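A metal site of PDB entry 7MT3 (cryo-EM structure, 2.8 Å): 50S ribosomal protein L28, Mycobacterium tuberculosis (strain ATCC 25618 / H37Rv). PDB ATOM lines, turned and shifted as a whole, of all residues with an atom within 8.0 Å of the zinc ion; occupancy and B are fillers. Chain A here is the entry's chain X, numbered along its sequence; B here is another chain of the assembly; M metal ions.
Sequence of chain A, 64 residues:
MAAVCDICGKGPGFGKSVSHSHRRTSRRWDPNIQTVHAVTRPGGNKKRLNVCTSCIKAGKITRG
The side-chain sulfur of Cys 5 sits close to the backbone NH of Ile 7 (3.6 Å). The backbone carbonyl oxygen of Lys 10 sits at hydrogen-bond distance from the backbone NH of Cys 5, at 3.3 Å. The side-chain hydroxyl of Ser 54 sits close to the side-chain sulfur of Cys 52. SG of Cys 8 lies close to N of Lys 10.
Along chain A the residues within 4 Å of the zinc ion span positions 5 to 55.
The zinc ion is bound by SG of Cys 5 (2.5 Å), SG of Cys 8 (2.5 Å), SG of Cys 52 (2.5 Å) and SG of Cys 55 (2.5 Å). The zinc ion has four donor atoms within binding distance.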
ATOM      1  N   VAL A   4      20.923 -22.215  -7.424  1.00  0.00           N
ATOM      2  CA  VAL A   4      21.925 -23.143  -7.925  1.00  0.00           C
ATOM      3  C   VAL A   4      21.244 -24.479  -8.138  1.00  0.00           C
ATOM      4  O   VAL A   4      20.650 -25.023  -7.209  1.00  0.00           O
ATOM      5  CB  VAL A   4      23.105 -23.307  -6.967  1.00  0.00           C
ATOM      6  CG1 VAL A   4      24.043 -24.370  -7.457  1.00  0.00           C
ATOM      7  CG2 VAL A   4      23.850 -22.001  -6.810  1.00  0.00           C
ATOM      8  N   CYS A   5      21.339 -25.015  -9.352  1.00  0.00           N
ATOM      9  CA  CYS A   5      20.791 -26.333  -9.618  1.00  0.00           C
ATOM     10  C   CYS A   5      21.661 -27.385  -8.949  1.00  0.00           C
ATOM     11  O   CYS A   5      22.887 -27.321  -8.992  1.00  0.00           O
ATOM     12  CB  CYS A   5      20.716 -26.601 -11.113  1.00  0.00           C
ATOM     13  SG  CYS A   5      19.920 -28.154 -11.558  1.00  0.00           S
ATOM     14  N   ASP A   6      21.014 -28.363  -8.311  1.00  0.00           N
ATOM     15  CA  ASP A   6      21.738 -29.401  -7.590  1.00  0.00           C
ATOM     16  C   ASP A   6      22.229 -30.526  -8.487  1.00  0.00           C
ATOM     17  O   ASP A   6      22.865 -31.449  -7.983  1.00  0.00           O
ATOM     18  CB  ASP A   6      20.875 -29.999  -6.483  1.00  0.00           C
ATOM     19  CG  ASP A   6      20.782 -29.088  -5.271  1.00  0.00           C
ATOM     20  OD1 ASP A   6      21.724 -28.300  -5.056  1.00  0.00           O
ATOM     21  OD2 ASP A   6      19.777 -29.179  -4.545  1.00  0.00           O
ATOM     22  N   ILE A   7      21.964 -30.479  -9.797  1.00  0.00           N
ATOM     23  CA  ILE A   7      22.399 -31.518 -10.715  1.00  0.00           C
ATOM     24  C   ILE A   7      23.411 -30.982 -11.726  1.00  0.00           C
ATOM     25  O   ILE A   7      24.545 -31.458 -11.775  1.00  0.00           O
ATOM     26  CB  ILE A   7      21.184 -32.166 -11.431  1.00  0.00           C
ATOM     27  CG1 ILE A   7      20.314 -32.864 -10.405  1.00  0.00           C
ATOM     28  CG2 ILE A   7      21.643 -33.140 -12.479  1.00  0.00           C
ATOM     29  CD1 ILE A   7      19.039 -33.305 -10.970  1.00  0.00           C
ATOM     30  N   CYS A   8      23.018 -30.004 -12.527  1.00  0.00           N
ATOM     31  CA  CYS A   8      23.887 -29.496 -13.578  1.00  0.00           C
ATOM     32  C   CYS A   8      24.722 -28.303 -13.140  1.00  0.00           C
ATOM     33  O   CYS A   8      25.535 -27.816 -13.938  1.00  0.00           O
ATOM     34  CB  CYS A   8      23.065 -29.123 -14.813  1.00  0.00           C
ATOM     35  SG  CYS A   8      21.911 -27.770 -14.588  1.00  0.00           S
ATOM     36  N   GLY A   9      24.548 -27.814 -11.924  1.00  0.00           N
ATOM     37  CA  GLY A   9      25.382 -26.731 -11.433  1.00  0.00           C
ATOM     38  C   GLY A   9      25.099 -25.373 -12.021  1.00  0.00           C
ATOM     39  O   GLY A   9      25.911 -24.468 -11.854  1.00  0.00           O
ATOM     40  N   LYS A  10      23.977 -25.204 -12.709  1.00  0.00           N
ATOM     41  CA  LYS A  10      23.643 -23.944 -13.376  1.00  0.00           C
ATOM     42  C   LYS A  10      23.306 -22.881 -12.343  1.00  0.00           C
ATOM     43  O   LYS A  10      22.267 -22.942 -11.686  1.00  0.00           O
ATOM     44  CB  LYS A  10      22.489 -24.156 -14.340  1.00  0.00           C
ATOM     45  CG  LYS A  10      21.976 -22.910 -14.993  1.00  0.00           C
ATOM     46  CD  LYS A  10      21.260 -23.230 -16.285  1.00  0.00           C
ATOM     47  CE  LYS A  10      19.957 -23.909 -16.077  1.00  0.00           C
ATOM     48  NZ  LYS A  10      19.314 -24.063 -17.398  1.00  0.00           N
ATOM     49  N   PRO A  31      18.422 -18.543 -12.320  1.00  0.00           N
ATOM     50  CA  PRO A  31      17.748 -19.650 -13.006  1.00  0.00           C
ATOM     51  C   PRO A  31      16.399 -19.969 -12.379  1.00  0.00           C
ATOM     52  O   PRO A  31      16.068 -19.544 -11.281  1.00  0.00           O
ATOM     53  CB  PRO A  31      18.728 -20.802 -12.850  1.00  0.00           C
ATOM     54  CG  PRO A  31      19.496 -20.473 -11.665  1.00  0.00           C
ATOM     55  CD  PRO A  31      19.625 -18.998 -11.625  1.00  0.00           C
ATOM     56  N   ASN A  32      15.625 -20.760 -13.115  1.00  0.00           N
ATOM     57  CA  ASN A  32      14.270 -21.123 -12.726  1.00  0.00           C
ATOM     58  C   ASN A  32      14.339 -22.363 -11.847  1.00  0.00           C
ATOM     59  O   ASN A  32      14.023 -23.473 -12.261  1.00  0.00           O
ATOM     60  CB  ASN A  32      13.398 -21.347 -13.947  1.00  0.00           C
ATOM     61  CG  ASN A  32      11.932 -21.340 -13.625  1.00  0.00           C
ATOM     62  OD1 ASN A  32      11.531 -21.199 -12.480  1.00  0.00           O
ATOM     63  ND2 ASN A  32      11.115 -21.473 -14.643  1.00  0.00           N
ATOM     64  N   ILE A  33      14.774 -22.161 -10.618  1.00  0.00           N
ATOM     65  CA  ILE A  33      15.010 -23.253  -9.692  1.00  0.00           C
ATOM     66  C   ILE A  33      13.724 -23.586  -8.969  1.00  0.00           C
ATOM     67  O   ILE A  33      13.148 -22.737  -8.271  1.00  0.00           O
ATOM     68  CB  ILE A  33      16.128 -22.900  -8.702  1.00  0.00           C
ATOM     69  CG1 ILE A  33      17.462 -22.776  -9.437  1.00  0.00           C
ATOM     70  CG2 ILE A  33      16.201 -23.924  -7.624  1.00  0.00           C
ATOM     71  CD1 ILE A  33      17.879 -24.036 -10.119  1.00  0.00           C
ATOM     72  N   ASN A  50      16.768 -28.988  -5.143  1.00  0.00           N
ATOM     73  CA  ASN A  50      16.554 -27.795  -5.961  1.00  0.00           C
ATOM     74  C   ASN A  50      17.036 -28.101  -7.371  1.00  0.00           C
ATOM     75  O   ASN A  50      18.237 -28.300  -7.585  1.00  0.00           O
ATOM     76  CB  ASN A  50      17.320 -26.606  -5.399  1.00  0.00           C
ATOM     77  CG  ASN A  50      16.740 -26.092  -4.112  1.00  0.00           C
ATOM     78  OD1 ASN A  50      15.529 -26.074  -3.931  1.00  0.00           O
ATOM     79  ND2 ASN A  50      17.609 -25.661  -3.208  1.00  0.00           N
ATOM     80  N   VAL A  51      16.111 -28.174  -8.328  1.00  0.00           N
ATOM     81  CA  VAL A  51      16.481 -28.405  -9.725  1.00  0.00           C
ATOM     82  C   VAL A  51      15.916 -27.267 -10.565  1.00  0.00           C
ATOM     83  O   VAL A  51      15.011 -26.550 -10.162  1.00  0.00           O
ATOM     84  CB  VAL A  51      15.986 -29.758 -10.254  1.00  0.00           C
ATOM     85  CG1 VAL A  51      16.599 -30.880  -9.477  1.00  0.00           C
ATOM     86  CG2 VAL A  51      14.523 -29.815 -10.136  1.00  0.00           C
ATOM     87  N   CYS A  52      16.466 -27.133 -11.761  1.00  0.00           N
ATOM     88  CA  CYS A  52      16.008 -26.114 -12.694  1.00  0.00           C
ATOM     89  C   CYS A  52      14.976 -26.712 -13.628  1.00  0.00           C
ATOM     90  O   CYS A  52      14.854 -27.927 -13.756  1.00  0.00           O
ATOM     91  CB  CYS A  52      17.175 -25.532 -13.485  1.00  0.00           C
ATOM     92  SG  CYS A  52      17.972 -26.677 -14.605  1.00  0.00           S
ATOM     93  N   THR A  53      14.207 -25.835 -14.274  1.00  0.00           N
ATOM     94  CA  THR A  53      13.100 -26.329 -15.083  1.00  0.00           C
ATOM     95  C   THR A  53      13.549 -26.924 -16.393  1.00  0.00           C
ATOM     96  O   THR A  53      12.772 -27.646 -17.030  1.00  0.00           O
ATOM     97  CB  THR A  53      12.102 -25.211 -15.357  1.00  0.00           C
ATOM     98  OG1 THR A  53      12.790 -24.096 -15.927  1.00  0.00           O
ATOM     99  CG2 THR A  53      11.413 -24.803 -14.093  1.00  0.00           C
ATOM    100  N   SER A  54      14.766 -26.667 -16.828  1.00  0.00           N
ATOM    101  CA  SER A  54      15.274 -27.315 -18.027  1.00  0.00           C
ATOM    102  C   SER A  54      15.715 -28.751 -17.771  1.00  0.00           C
ATOM    103  O   SER A  54      16.064 -29.457 -18.717  1.00  0.00           O
ATOM    104  CB  SER A  54      16.424 -26.509 -18.612  1.00  0.00           C
ATOM    105  OG  SER A  54      17.520 -26.504 -17.726  1.00  0.00           O
ATOM    106  N   CYS A  55      15.730 -29.193 -16.512  1.00  0.00           N
ATOM    107  CA  CYS A  55      15.968 -30.583 -16.170  1.00  0.00           C
ATOM    108  C   CYS A  55      14.713 -31.342 -15.812  1.00  0.00           C
ATOM    109  O   CYS A  55      14.667 -32.568 -15.984  1.00  0.00           O
ATOM    110  CB  CYS A  55      16.961 -30.679 -15.012  1.00  0.00           C
ATOM    111  SG  CYS A  55      18.624 -30.133 -15.427  1.00  0.00           S
ATOM    112  N   ILE A  56      13.676 -30.654 -15.326  1.00  0.00           N
ATOM    113  CA  ILE A  56      12.381 -31.300 -15.146  1.00  0.00           C
ATOM    114  C   ILE A  56      11.750 -31.555 -16.500  1.00  0.00           C
ATOM    115  O   ILE A  56      11.009 -32.520 -16.677  1.00  0.00           O
ATOM    116  CB  ILE A  56      11.484 -30.433 -14.253  1.00  0.00           C
ATOM    117  CG1 ILE A  56      12.212 -30.053 -12.974  1.00  0.00           C
ATOM    118  CG2 ILE A  56      10.253 -31.168 -13.832  1.00  0.00           C
ATOM    119  CD1 ILE A  56      11.509 -28.980 -12.209  1.00  0.00           C
ATOM    120  N   LYS A  60      16.004 -35.897 -16.112  1.00  0.00           N
ATOM    121  CA  LYS A  60      17.118 -35.993 -15.187  1.00  0.00           C
ATOM    122  C   LYS A  60      16.688 -36.483 -13.808  1.00  0.00           C
ATOM    123  O   LYS A  60      17.510 -37.045 -13.084  1.00  0.00           O
ATOM    124  CB  LYS A  60      17.810 -34.647 -15.039  1.00  0.00           C
ATOM    125  CG  LYS A  60      18.384 -34.025 -16.316  1.00  0.00           C
ATOM    126  CD  LYS A  60      19.722 -34.617 -16.747  1.00  0.00           C
ATOM    127  CE  LYS A  60      19.578 -35.566 -17.914  1.00  0.00           C
ATOM    128  NZ  LYS A  60      20.907 -35.996 -18.406  1.00  0.00           N
ATOM    129  P     U B 486      17.333 -20.611 -16.915  1.00  0.00           P
ATOM    130  OP1   U B 486      16.964 -21.458 -15.768  1.00  0.00           O
ATOM    131  OP2   U B 486      18.134 -21.178 -18.008  1.00  0.00           O
ATOM    132  O5'   U B 486      16.006 -20.007 -17.558  1.00  0.00           O
ATOM    133  C5'   U B 486      15.061 -19.315 -16.760  1.00  0.00           C
ATOM    134  C4'   U B 486      13.976 -18.690 -17.591  1.00  0.00           C
ATOM    135  O4'   U B 486      14.530 -17.632 -18.409  1.00  0.00           O
ATOM    136  C3'   U B 486      13.288 -19.594 -18.603  1.00  0.00           C
ATOM    137  O3'   U B 486      12.297 -20.422 -18.023  1.00  0.00           O
ATOM    138  C2'   U B 486      12.726 -18.588 -19.595  1.00  0.00           C
ATOM    139  O2'   U B 486      11.569 -17.962 -19.089  1.00  0.00           O
ATOM    140  C1'   U B 486      13.842 -17.556 -19.632  1.00  0.00           C
ATOM    141  N1    U B 486      14.812 -17.793 -20.728  1.00  0.00           N
ATOM    142  C2    U B 486      14.471 -17.402 -22.004  1.00  0.00           C
ATOM    143  O2    U B 486      13.424 -16.871 -22.284  1.00  0.00           O
ATOM    144  N3    U B 486      15.406 -17.663 -22.958  1.00  0.00           N
ATOM    145  C4    U B 486      16.628 -18.242 -22.787  1.00  0.00           C
ATOM    146  O4    U B 486      17.373 -18.421 -23.739  1.00  0.00           O
ATOM    147  C5    U B 486      16.919 -18.619 -21.453  1.00  0.00           C
ATOM    148  C6    U B 486      16.020 -18.381 -20.502  1.00  0.00           C
HETATM  149 ZN    ZN M   1      19.618 -28.396 -13.978  1.00  0.00          ZN
